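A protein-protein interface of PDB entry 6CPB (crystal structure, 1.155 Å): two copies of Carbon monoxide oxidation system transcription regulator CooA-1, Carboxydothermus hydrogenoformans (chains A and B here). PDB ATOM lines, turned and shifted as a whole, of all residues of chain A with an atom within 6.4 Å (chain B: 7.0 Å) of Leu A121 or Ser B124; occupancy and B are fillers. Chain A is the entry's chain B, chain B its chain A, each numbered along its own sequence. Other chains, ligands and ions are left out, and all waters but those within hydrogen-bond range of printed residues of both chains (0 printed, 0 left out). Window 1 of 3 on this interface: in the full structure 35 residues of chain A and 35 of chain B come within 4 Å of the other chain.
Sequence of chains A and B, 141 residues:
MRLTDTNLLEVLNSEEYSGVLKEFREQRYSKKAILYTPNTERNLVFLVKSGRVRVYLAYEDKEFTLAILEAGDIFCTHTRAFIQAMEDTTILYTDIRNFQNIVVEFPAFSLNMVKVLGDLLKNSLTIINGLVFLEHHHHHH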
ATOM      1  N   VAL A 116      -2.117 -14.877  21.022  1.00  0.00           N
ATOM      2  CA  VAL A 116      -2.410 -14.772  22.452  1.00  0.00           C
ATOM      3  C   VAL A 116      -3.071 -13.435  22.759  1.00  0.00           C
ATOM      4  O   VAL A 116      -4.101 -13.370  23.442  1.00  0.00           O
ATOM      5  CB  VAL A 116      -1.127 -14.990  23.283  1.00  0.00           C
ATOM      6  CG1 VAL A 116      -1.384 -14.741  24.765  1.00  0.00           C
ATOM      7  CG2 VAL A 116      -0.587 -16.398  23.079  1.00  0.00           C
ATOM      8  N   LEU A 117      -2.497 -12.346  22.256  1.00  0.00           N
ATOM      9  CA  LEU A 117      -3.044 -11.028  22.553  1.00  0.00           C
ATOM     10  C   LEU A 117      -4.446 -10.877  21.993  1.00  0.00           C
ATOM     11  O   LEU A 117      -5.326 -10.314  22.655  1.00  0.00           O
ATOM     12  CB  LEU A 117      -2.145  -9.930  21.999  1.00  0.00           C
ATOM     13  CG  LEU A 117      -0.790  -9.747  22.667  1.00  0.00           C
ATOM     14  CD1 LEU A 117       0.026  -8.701  21.938  1.00  0.00           C
ATOM     15  CD2 LEU A 117      -0.940  -9.393  24.149  1.00  0.00           C
ATOM     16  N   GLY A 118      -4.675 -11.361  20.774  1.00  0.00           N
ATOM     17  CA  GLY A 118      -6.008 -11.298  20.208  1.00  0.00           C
ATOM     18  C   GLY A 118      -7.007 -12.093  21.024  1.00  0.00           C
ATOM     19  O   GLY A 118      -8.138 -11.655  21.236  1.00  0.00           O
ATOM     20  N   ASP A 119      -6.599 -13.267  21.508  1.00  0.00           N
ATOM     21  CA  ASP A 119      -7.489 -14.090  22.323  1.00  0.00           C
ATOM     22  C   ASP A 119      -7.833 -13.392  23.631  1.00  0.00           C
ATOM     23  O   ASP A 119      -8.995 -13.369  24.055  1.00  0.00           O
ATOM     24  CB  ASP A 119      -6.829 -15.438  22.614  1.00  0.00           C
ATOM     25  CG  ASP A 119      -6.817 -16.364  21.416  1.00  0.00           C
ATOM     26  OD1 ASP A 119      -7.497 -16.063  20.411  1.00  0.00           O
ATOM     27  OD2 ASP A 119      -6.116 -17.399  21.484  1.00  0.00           O
ATOM     28  N   LEU A 120      -6.829 -12.829  24.298  1.00  0.00           N
ATOM     29  CA  LEU A 120      -7.082 -12.146  25.558  1.00  0.00           C
ATOM     30  C   LEU A 120      -7.902 -10.881  25.343  1.00  0.00           C
ATOM     31  O   LEU A 120      -8.786 -10.573  26.149  1.00  0.00           O
ATOM     32  CB  LEU A 120      -5.773 -11.855  26.285  1.00  0.00           C
ATOM     33  CG  LEU A 120      -5.292 -13.016  27.172  1.00  0.00           C
ATOM     34  CD1 LEU A 120      -4.964 -14.263  26.359  1.00  0.00           C
ATOM     35  CD2 LEU A 120      -4.089 -12.594  27.985  1.00  0.00           C
ATOM     36  N   LEU A 121      -7.648 -10.149  24.256  1.00  0.00           N
ATOM     37  CA  LEU A 121      -8.461  -8.980  23.943  1.00  0.00           C
ATOM     38  C   LEU A 121      -9.915  -9.380  23.751  1.00  0.00           C
ATOM     39  O   LEU A 121     -10.818  -8.774  24.332  1.00  0.00           O
ATOM     40  CB  LEU A 121      -7.921  -8.263  22.703  1.00  0.00           C
ATOM     41  CG  LEU A 121      -8.769  -7.073  22.234  1.00  0.00           C
ATOM     42  CD1 LEU A 121      -8.832  -5.982  23.308  1.00  0.00           C
ATOM     43  CD2 LEU A 121      -8.194  -6.501  20.963  1.00  0.00           C
ATOM     44  N   LYS A 122     -10.161 -10.396  22.935  1.00  0.00           N
ATOM     45  CA  LYS A 122     -11.534 -10.833  22.718  1.00  0.00           C
ATOM     46  C   LYS A 122     -12.193 -11.229  24.026  1.00  0.00           C
ATOM     47  O   LYS A 122     -13.350 -10.856  24.298  1.00  0.00           O
ATOM     48  CB  LYS A 122     -11.528 -12.018  21.765  1.00  0.00           C
ATOM     49  CG  LYS A 122     -11.300 -11.604  20.342  1.00  0.00           C
ATOM     50  CD  LYS A 122     -11.177 -12.801  19.388  1.00  0.00           C
ATOM     51  CE  LYS A 122     -12.524 -13.242  18.846  1.00  0.00           C
ATOM     52  NZ  LYS A 122     -12.390 -14.231  17.725  1.00  0.00           N
ATOM     53  N   ASN A 123     -11.470 -11.969  24.864  1.00  0.00           N
ATOM     54  CA  ASN A 123     -12.015 -12.371  26.154  1.00  0.00           C
ATOM     55  C   ASN A 123     -12.395 -11.145  26.962  1.00  0.00           C
ATOM     56  O   ASN A 123     -13.495 -11.068  27.511  1.00  0.00           O
ATOM     57  CB  ASN A 123     -10.988 -13.228  26.903  1.00  0.00           C
ATOM     58  CG  ASN A 123     -11.531 -13.771  28.196  1.00  0.00           C
ATOM     59  OD1 ASN A 123     -12.734 -13.793  28.395  1.00  0.00           O
ATOM     60  ND2 ASN A 123     -10.649 -14.249  29.067  1.00  0.00           N
ATOM     61  N   SER A 124     -11.510 -10.153  26.991  1.00  0.00           N
ATOM     62  CA  SER A 124     -11.739  -8.973  27.803  1.00  0.00           C
ATOM     63  C   SER A 124     -12.954  -8.191  27.320  1.00  0.00           C
ATOM     64  O   SER A 124     -13.695  -7.631  28.134  1.00  0.00           O
ATOM     65  CB  SER A 124     -10.493  -8.098  27.836  1.00  0.00           C
ATOM     66  OG  SER A 124     -10.282  -7.426  26.622  1.00  0.00           O
ATOM     67  N   LEU A 125     -13.176  -8.137  26.005  1.00  0.00           N
ATOM     68  CA  LEU A 125     -14.350  -7.440  25.492  1.00  0.00           C
ATOM     69  C   LEU A 125     -15.643  -8.162  25.879  1.00  0.00           C
ATOM     70  O   LEU A 125     -16.648  -7.507  26.198  1.00  0.00           O
ATOM     71  CB  LEU A 125     -14.217  -7.187  23.992  1.00  0.00           C
ATOM     72  CG  LEU A 125     -13.000  -6.337  23.570  1.00  0.00           C
ATOM     73  CD1 LEU A 125     -13.058  -6.073  22.077  1.00  0.00           C
ATOM     74  CD2 LEU A 125     -12.856  -5.027  24.324  1.00  0.00           C
ATOM     75  N   THR A 126     -15.638  -9.515  25.871  1.00  0.00           N
ATOM     76  CA  THR A 126     -16.797 -10.260  26.380  1.00  0.00           C
ATOM     77  C   THR A 126     -17.043  -9.927  27.838  1.00  0.00           C
ATOM     78  O   THR A 126     -18.194  -9.749  28.263  1.00  0.00           O
ATOM     79  CB  THR A 126     -16.699 -11.803  26.204  1.00  0.00           C
ATOM     80  OG1 THR A 126     -15.811 -12.433  27.164  1.00  0.00           O
ATOM     81  CG2 THR A 126     -16.298 -12.182  24.788  1.00  0.00           C
ATOM     82  N   ILE A 128     -16.357  -7.180  29.441  1.00  0.00           N
ATOM     83  CA  ILE A 128     -16.989  -5.861  29.509  1.00  0.00           C
ATOM     84  C   ILE A 128     -18.479  -5.965  29.199  1.00  0.00           C
ATOM     85  O   ILE A 128     -19.314  -5.423  29.928  1.00  0.00           O
ATOM     86  CB  ILE A 128     -16.268  -4.861  28.585  1.00  0.00           C
ATOM     87  CG1 ILE A 128     -14.866  -4.580  29.114  1.00  0.00           C
ATOM     88  CG2 ILE A 128     -17.080  -3.562  28.470  1.00  0.00           C
ATOM     89  CD1 ILE A 128     -13.962  -3.842  28.131  1.00  0.00           C
ATOM     90  N   VAL B  55     -11.041   2.624  17.484  1.00  0.00           N
ATOM     91  CA  VAL B  55     -11.487   1.277  17.812  1.00  0.00           C
ATOM     92  C   VAL B  55     -12.312   1.391  19.083  1.00  0.00           C
ATOM     93  O   VAL B  55     -11.868   2.013  20.053  1.00  0.00           O
ATOM     94  CB  VAL B  55     -10.292   0.333  18.024  1.00  0.00           C
ATOM     95  CG1 VAL B  55     -10.771  -1.068  18.309  1.00  0.00           C
ATOM     96  CG2 VAL B  55      -9.375   0.345  16.809  1.00  0.00           C
ATOM     97  N   THR B  65     -14.331   3.903  23.938  1.00  0.00           N
ATOM     98  CA  THR B  65     -13.196   3.922  23.033  1.00  0.00           C
ATOM     99  C   THR B  65     -12.081   3.059  23.603  1.00  0.00           C
ATOM    100  O   THR B  65     -11.735   3.163  24.781  1.00  0.00           O
ATOM    101  CB  THR B  65     -12.724   5.351  22.833  1.00  0.00           C
ATOM    102  OG1 THR B  65     -13.800   6.069  22.235  1.00  0.00           O
ATOM    103  CG2 THR B  65     -11.475   5.423  21.959  1.00  0.00           C
ATOM    104  N   LEU B  66     -11.533   2.191  22.763  1.00  0.00           N
ATOM    105  CA  LEU B  66     -10.461   1.281  23.140  1.00  0.00           C
ATOM    106  C   LEU B  66      -9.089   1.772  22.714  1.00  0.00           C
ATOM    107  O   LEU B  66      -8.112   1.540  23.421  1.00  0.00           O
ATOM    108  CB  LEU B  66     -10.729  -0.099  22.540  1.00  0.00           C
ATOM    109  CG  LEU B  66     -12.012  -0.795  22.994  1.00  0.00           C
ATOM    110  CD1 LEU B  66     -12.325  -2.013  22.133  1.00  0.00           C
ATOM    111  CD2 LEU B  66     -11.932  -1.164  24.454  1.00  0.00           C
ATOM    112  N   PHE B  75      -4.406  -3.310  12.366  1.00  0.00           N
ATOM    113  CA  PHE B  75      -5.366  -3.993  13.238  1.00  0.00           C
ATOM    114  C   PHE B  75      -6.102  -5.037  12.389  1.00  0.00           C
ATOM    115  O   PHE B  75      -5.654  -5.377  11.290  1.00  0.00           O
ATOM    116  CB  PHE B  75      -6.234  -2.953  13.974  1.00  0.00           C
ATOM    117  CG  PHE B  75      -7.158  -3.528  15.040  1.00  0.00           C
ATOM    118  CD1 PHE B  75      -6.715  -4.455  15.977  1.00  0.00           C
ATOM    119  CD2 PHE B  75      -8.480  -3.128  15.084  1.00  0.00           C
ATOM    120  CE1 PHE B  75      -7.587  -4.981  16.916  1.00  0.00           C
ATOM    121  CE2 PHE B  75      -9.343  -3.633  16.029  1.00  0.00           C
ATOM    122  CZ  PHE B  75      -8.893  -4.555  16.952  1.00  0.00           C
ATOM    123  N   CYS B  76      -7.211  -5.576  12.896  1.00  0.00           N
ATOM    124  CA  CYS B  76      -7.846  -6.696  12.233  1.00  0.00           C
ATOM    125  C   CYS B  76      -9.297  -6.794  12.675  1.00  0.00           C
ATOM    126  O   CYS B  76      -9.697  -6.253  13.714  1.00  0.00           O
ATOM    127  CB  CYS B  76      -7.113  -7.988  12.570  1.00  0.00           C
ATOM    128  SG  CYS B  76      -6.906  -8.246  14.354  1.00  0.00           S
ATOM    129  N   THR B  79     -12.216  -9.364  16.084  1.00  0.00           N
ATOM    130  CA  THR B  79     -11.742  -8.979  17.408  1.00  0.00           C
ATOM    131  C   THR B  79     -12.829  -8.272  18.216  1.00  0.00           C
ATOM    132  O   THR B  79     -12.518  -7.524  19.152  1.00  0.00           O
ATOM    133  CB  THR B  79     -10.487  -8.116  17.269  1.00  0.00           C
ATOM    134  OG1 THR B  79     -10.768  -7.020  16.387  1.00  0.00           O
ATOM    135  CG2 THR B  79      -9.337  -8.946  16.695  1.00  0.00           C
ATOM    136  N   ARG B  80     -14.095  -8.503  17.868  1.00  0.00           N
ATOM    137  CA  ARG B  80     -15.241  -8.069  18.669  1.00  0.00           C
ATOM    138  C   ARG B  80     -15.326  -6.551  18.821  1.00  0.00           C
ATOM    139  O   ARG B  80     -15.947  -6.047  19.759  1.00  0.00           O
ATOM    140  CB  ARG B  80     -15.301  -8.777  20.028  1.00  0.00           C
ATOM    141  CG  ARG B  80     -15.376 -10.287  19.914  1.00  0.00           C
ATOM    142  CD  ARG B  80     -15.593 -10.918  21.277  1.00  0.00           C
ATOM    143  NE  ARG B  80     -14.997 -12.250  21.358  1.00  0.00           N
ATOM    144  CZ  ARG B  80     -15.654 -13.405  21.294  1.00  0.00           C
ATOM    145  NH1 ARG B  80     -16.972 -13.442  21.153  1.00  0.00           N
ATOM    146  NH2 ARG B  80     -14.974 -14.542  21.381  1.00  0.00           N
ATOM    147  N   ALA B  81     -14.770  -5.807  17.872  1.00  0.00           N
ATOM    148  CA  ALA B  81     -14.665  -4.360  17.980  1.00  0.00           C
ATOM    149  C   ALA B  81     -15.283  -3.663  16.774  1.00  0.00           C
ATOM    150  O   ALA B  81     -15.352  -4.215  15.670  1.00  0.00           O
ATOM    151  CB  ALA B  81     -13.203  -3.947  18.092  1.00  0.00           C
ATOM    152  N   VAL B 116      -0.140  -2.547  18.868  1.00  0.00           N
ATOM    153  CA  VAL B 116      -1.545  -2.133  18.849  1.00  0.00           C
ATOM    154  C   VAL B 116      -2.391  -3.043  19.734  1.00  0.00           C
ATOM    155  O   VAL B 116      -3.189  -2.568  20.561  1.00  0.00           O
ATOM    156  CB  VAL B 116      -2.071  -2.104  17.399  1.00  0.00           C
ATOM    157  CG1 VAL B 116      -3.584  -1.977  17.370  1.00  0.00           C
ATOM    158  CG2 VAL B 116      -1.430  -0.978  16.599  1.00  0.00           C
ATOM    159  N   LEU B 117      -2.233  -4.364  19.583  1.00  0.00           N
ATOM    160  CA  LEU B 117      -3.027  -5.294  20.380  1.00  0.00           C
ATOM    161  C   LEU B 117      -2.703  -5.158  21.856  1.00  0.00           C
ATOM    162  O   LEU B 117      -3.598  -5.253  22.705  1.00  0.00           O
ATOM    163  CB  LEU B 117      -2.803  -6.730  19.910  1.00  0.00           C
ATOM    164  CG  LEU B 117      -3.405  -7.092  18.549  1.00  0.00           C
ATOM    165  CD1 LEU B 117      -2.941  -8.473  18.133  1.00  0.00           C
ATOM    166  CD2 LEU B 117      -4.913  -7.023  18.529  1.00  0.00           C
ATOM    167  N   GLY B 118      -1.426  -4.956  22.187  1.00  0.00           N
ATOM    168  CA  GLY B 118      -1.059  -4.768  23.578  1.00  0.00           C
ATOM    169  C   GLY B 118      -1.708  -3.537  24.179  1.00  0.00           C
ATOM    170  O   GLY B 118      -2.171  -3.565  25.322  1.00  0.00           O
ATOM    171  N   ASP B 119      -1.756  -2.439  23.415  1.00  0.00           N
ATOM    172  CA  ASP B 119      -2.410  -1.219  23.889  1.00  0.00           C
ATOM    173  C   ASP B 119      -3.917  -1.418  24.035  1.00  0.00           C
ATOM    174  O   ASP B 119      -4.514  -0.969  25.027  1.00  0.00           O
ATOM    175  CB  ASP B 119      -2.134  -0.056  22.934  1.00  0.00           C
ATOM    176  CG  ASP B 119      -0.758   0.541  23.104  1.00  0.00           C
ATOM    177  OD1 ASP B 119      -0.117   0.300  24.153  1.00  0.00           O
ATOM    178  OD2 ASP B 119      -0.324   1.272  22.185  1.00  0.00           O
ATOM    179  N   LEU B 120      -4.546  -2.087  23.063  1.00  0.00           N
ATOM    180  CA  LEU B 120      -5.977  -2.356  23.159  1.00  0.00           C
ATOM    181  C   LEU B 120      -6.292  -3.201  24.382  1.00  0.00           C
ATOM    182  O   LEU B 120      -7.265  -2.930  25.102  1.00  0.00           O
ATOM    183  CB  LEU B 120      -6.446  -3.069  21.895  1.00  0.00           C
ATOM    184  CG  LEU B 120      -6.590  -2.170  20.670  1.00  0.00           C
ATOM    185  CD1 LEU B 120      -6.657  -3.022  19.415  1.00  0.00           C
ATOM    186  CD2 LEU B 120      -7.841  -1.318  20.787  1.00  0.00           C
ATOM    187  N   LEU B 121      -5.486  -4.233  24.634  1.00  0.00           N
ATOM    188  CA  LEU B 121      -5.722  -5.090  25.785  1.00  0.00           C
ATOM    189  C   LEU B 121      -5.513  -4.323  27.085  1.00  0.00           C
ATOM    190  O   LEU B 121      -6.321  -4.423  28.012  1.00  0.00           O
ATOM    191  CB  LEU B 121      -4.826  -6.328  25.719  1.00  0.00           C
ATOM    192  CG  LEU B 121      -4.964  -7.292  26.897  1.00  0.00           C
ATOM    193  CD1 LEU B 121      -6.372  -7.860  27.017  1.00  0.00           C
ATOM    194  CD2 LEU B 121      -3.928  -8.412  26.761  1.00  0.00           C
ATOM    195  N   LYS B 122      -4.427  -3.558  27.182  1.00  0.00           N
ATOM    196  CA  LYS B 122      -4.206  -2.712  28.348  1.00  0.00           C
ATOM    197  C   LYS B 122      -5.419  -1.821  28.610  1.00  0.00           C
ATOM    198  O   LYS B 122      -5.919  -1.723  29.737  1.00  0.00           O
ATOM    199  CB  LYS B 122      -2.948  -1.878  28.114  1.00  0.00           C
ATOM    200  CG  LYS B 122      -2.654  -0.863  29.203  1.00  0.00           C
ATOM    201  CD  LYS B 122      -1.419  -0.054  28.849  1.00  0.00           C
ATOM    202  CE  LYS B 122      -1.232   1.109  29.812  1.00  0.00           C
ATOM    203  NZ  LYS B 122      -1.098   0.657  31.222  1.00  0.00           N
ATOM    204  N   ASN B 123      -5.935  -1.195  27.559  1.00  0.00           N
ATOM    205  CA  ASN B 123      -7.042  -0.259  27.722  1.00  0.00           C
ATOM    206  C   ASN B 123      -8.341  -0.973  28.071  1.00  0.00           C
ATOM    207  O   ASN B 123      -9.157  -0.440  28.845  1.00  0.00           O
ATOM    208  CB  ASN B 123      -7.192   0.597  26.464  1.00  0.00           C
ATOM    209  CG  ASN B 123      -6.037   1.539  26.271  1.00  0.00           C
ATOM    210  OD1 ASN B 123      -5.215   1.724  27.174  1.00  0.00           O
ATOM    211  ND2 ASN B 123      -5.956   2.137  25.095  1.00  0.00           N
ATOM    212  N   SER B 124      -8.549  -2.186  27.554  1.00  0.00           N
ATOM    213  CA  SER B 124      -9.753  -2.937  27.897  1.00  0.00           C
ATOM    214  C   SER B 124      -9.728  -3.395  29.354  1.00  0.00           C
ATOM    215  O   SER B 124     -10.776  -3.433  30.015  1.00  0.00           O
ATOM    216  CB  SER B 124      -9.940  -4.117  26.937  1.00  0.00           C
ATOM    217  OG  SER B 124      -8.971  -5.121  27.154  1.00  0.00           O
ATOM    218  N   LEU B 125      -8.552  -3.745  29.880  1.00  0.00           N
ATOM    219  CA  LEU B 125      -8.473  -4.102  31.294  1.00  0.00           C
ATOM    220  C   LEU B 125      -8.706  -2.886  32.176  1.00  0.00           C
ATOM    221  O   LEU B 125      -9.299  -3.001  33.259  1.00  0.00           O
ATOM    222  CB  LEU B 125      -7.136  -4.756  31.626  1.00  0.00           C
ATOM    223  CG  LEU B 125      -6.813  -6.043  30.872  1.00  0.00           C
ATOM    224  CD1 LEU B 125      -5.629  -6.725  31.551  1.00  0.00           C
ATOM    225  CD2 LEU B 125      -7.987  -6.990  30.750  1.00  0.00           C
ATOM    226  N   THR B 126      -8.277  -1.709  31.719  1.00  0.00           N
ATOM    227  CA  THR B 126      -8.587  -0.480  32.434  1.00  0.00           C
ATOM    228  C   THR B 126     -10.094  -0.246  32.510  1.00  0.00           C
ATOM    229  O   THR B 126     -10.614   0.161  33.559  1.00  0.00           O
ATOM    230  CB  THR B 126      -7.845   0.680  31.779  1.00  0.00           C
ATOM    231  OG1 THR B 126      -6.446   0.463  31.995  1.00  0.00           O
ATOM    232  CG2 THR B 126      -8.248   2.034  32.350  1.00  0.00           C
ATOM    233  N   ILE B 127     -10.815  -0.510  31.417  1.00  0.00           N
ATOM    234  CA  ILE B 127     -12.271  -0.374  31.440  1.00  0.00           C
ATOM    235  C   ILE B 127     -12.886  -1.341  32.444  1.00  0.00           C
ATOM    236  O   ILE B 127     -13.759  -0.954  33.231  1.00  0.00           O
ATOM    237  CB  ILE B 127     -12.860  -0.547  30.029  1.00  0.00           C
ATOM    238  CG1 ILE B 127     -12.430   0.611  29.133  1.00  0.00           C
ATOM    239  CG2 ILE B 127     -14.389  -0.669  30.076  1.00  0.00           C
ATOM    240  CD1 ILE B 127     -12.496   0.295  27.649  1.00  0.00           C
ATOM    241  N   ILE B 128     -12.448  -2.607  32.434  1.00  0.00           N
ATOM    242  CA  ILE B 128     -12.968  -3.574  33.397  1.00  0.00           C
ATOM    243  C   ILE B 128     -12.738  -3.076  34.819  1.00  0.00           C
ATOM    244  O   ILE B 128     -13.644  -3.093  35.662  1.00  0.00           O
ATOM    245  CB  ILE B 128     -12.321  -4.952  33.175  1.00  0.00           C
ATOM    246  CG1 ILE B 128     -12.776  -5.555  31.844  1.00  0.00           C
ATOM    247  CG2 ILE B 128     -12.664  -5.890  34.336  1.00  0.00           C
ATOM    248  CD1 ILE B 128     -11.954  -6.752  31.403  1.00  0.00           C
ATOM    249  N   ASN B 129     -11.515  -2.636  35.100  1.00  0.00           N
ATOM    250  CA  ASN B 129     -11.160  -2.175  36.433  1.00  0.00           C
ATOM    251  C   ASN B 129     -12.063  -1.025  36.869  1.00  0.00           C
ATOM    252  O   ASN B 129     -12.483  -0.949  38.031  1.00  0.00           O
ATOM    253  CB  ASN B 129      -9.683  -1.763  36.419  1.00  0.00           C
ATOM    254  CG  ASN B 129      -9.119  -1.541  37.798  1.00  0.00           C
ATOM    255  OD1 ASN B 129      -8.978  -2.474  38.578  1.00  0.00           O
ATOM    256  ND2 ASN B 129      -8.797  -0.300  38.108  1.00  0.00           N
ATOM    257  N   GLY B 130     -12.385  -0.122  35.943  1.00  0.00           N
ATOM    258  CA  GLY B 130     -13.266   0.987  36.268  1.00  0.00           C
ATOM    259  C   GLY B 130     -14.701   0.560  36.496  1.00  0.00           C
ATOM    260  O   GLY B 130     -15.342   1.018  37.443  1.00  0.00           O
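The side-chain hydroxyl (OG) of Ser B124 is in hydrogen-bond range of the side-chain hydroxyl (OG) of Ser A124, 2.7 Å away.
O of Val B55 lies within hydrogen-bond range of N of Leu B66 (2.7 Å).
O of Leu B66 sits at hydrogen-bond distance from ND2 of Asn B123 (2.8 Å).
The side-chain hydroxyl (OG1) of Thr B79 sits at hydrogen-bond distance from the backbone carbonyl oxygen (O) of Cys B76, 3.0 Å away.
O of Leu B120 is in hydrogen-bond range of OG of Ser B124 (3.5 Å).
The backbone carbonyl oxygen (O) of Leu A121 is in hydrogen-bond range of the side-chain hydroxyl (OG) of Ser A124, 2.7 Å away.
OG1 of Thr A126 lies within hydrogen-bond range of O of Asn A123 (2.7 Å).
Printed residues of chain B within 4 Å of Leu A120: Leu B121 (3.7 Å).
Of the printed residues of chain B, Leu A121 touches Leu B120, Leu B121 and Ser B124.
Of the printed residues of chain B, Lys A122 touches Thr B79 (3.96 Å) and Arg B80 (3.5 Å).
Printed residues of chain B within 4 Å of Ile A128: Ser B124 (3.7 Å), Ile B127 (3.7 Å) and Ile B128 (3.6 Å).
Cys B76 touches none of the printed residues of chain A.
Of the printed residues of chain A, Thr B79 touches Lys A122 (3.96 Å) and Leu A125 (3.3 Å).
Ala B81 touches none of the printed residues of chain A.
Of the printed residues of chain A, Leu B117 touches Leu A117 (3.9 Å).
Of the printed residues of chain A, Ser B124 touches Leu A121, Ser A124 and Ile A128.
The nearest printed residue of chain A that does not touch Ser B124 is Leu A125 (4.02 Å).
The nearest printed residue of chain B that does not touch Ile A128 is Leu B66 (5.0 Å).
Of the 23 printed residues of chain B, 10 touch a printed residue of chain A.
Printed residues of chain B that touch a printed residue of chain A: Leu B66, Thr B79, Arg B80, Leu B117, Leu B120, Leu B121, Ser B124, Leu B125, Ile B127 and Ile B128.
Hydrophobic or aromatic side chains of chain B that line the printed part of chain A: Leu B66, Leu B117, Leu B120, Leu B121, Leu B125, Ile B127 and Ile B128.
Of the 12 printed residues of chain A, 8 touch a printed residue of chain B.
Printed residues of chain A that touch a printed residue of chain B: Leu A117, Leu A120, Leu A121, Lys A122, Ser A124, Leu A125, Thr A126 and Ile A128.
Hydrophobic or aromatic side chains of chain A within 4 Å of the printed part of chain B: Leu A117, Leu A120, Leu A121, Leu A125 and Ile A128.
Among the printed residues, no Asp or Glu carboxylate lies within 4 Å of a Lys or Arg side-chain nitrogen of the other chain.
Leu B117 touches its own counterpart, Leu A117.
Leu B121 touches its own counterpart, Leu A121.
Leu A121 touches Ser B124, and with the chains exchanged Ser A124 touches Leu B121.
Ser A124 touches Ile B128, and with the chains exchanged Ile A128 touches Ser B124.
Of the 18 pairs that touch across the chains among the printed residues, 10 have their exchanged pair printed and touching as well.
Among the printed residues, pairs that only touch across the chains: Leu A125 with Thr B79, Lys A122 with Arg B80, Ile A128 with Ile B128, Thr A126 with Arg B80, Leu A125 with Arg B80, Ile A128 with Ser B124, Leu A120 with Leu B121, Ile A128 with Ile B127, Leu A125 with Leu B66, Ser A124 with Ile B128, Leu A121 with Leu B121, Leu A121 with Leu B120, Leu A117 with Leu B117, Leu A121 with Ser B124, Ser A124 with Leu B121, Lys A122 with Thr B79 and Ser A124 with Leu B125.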
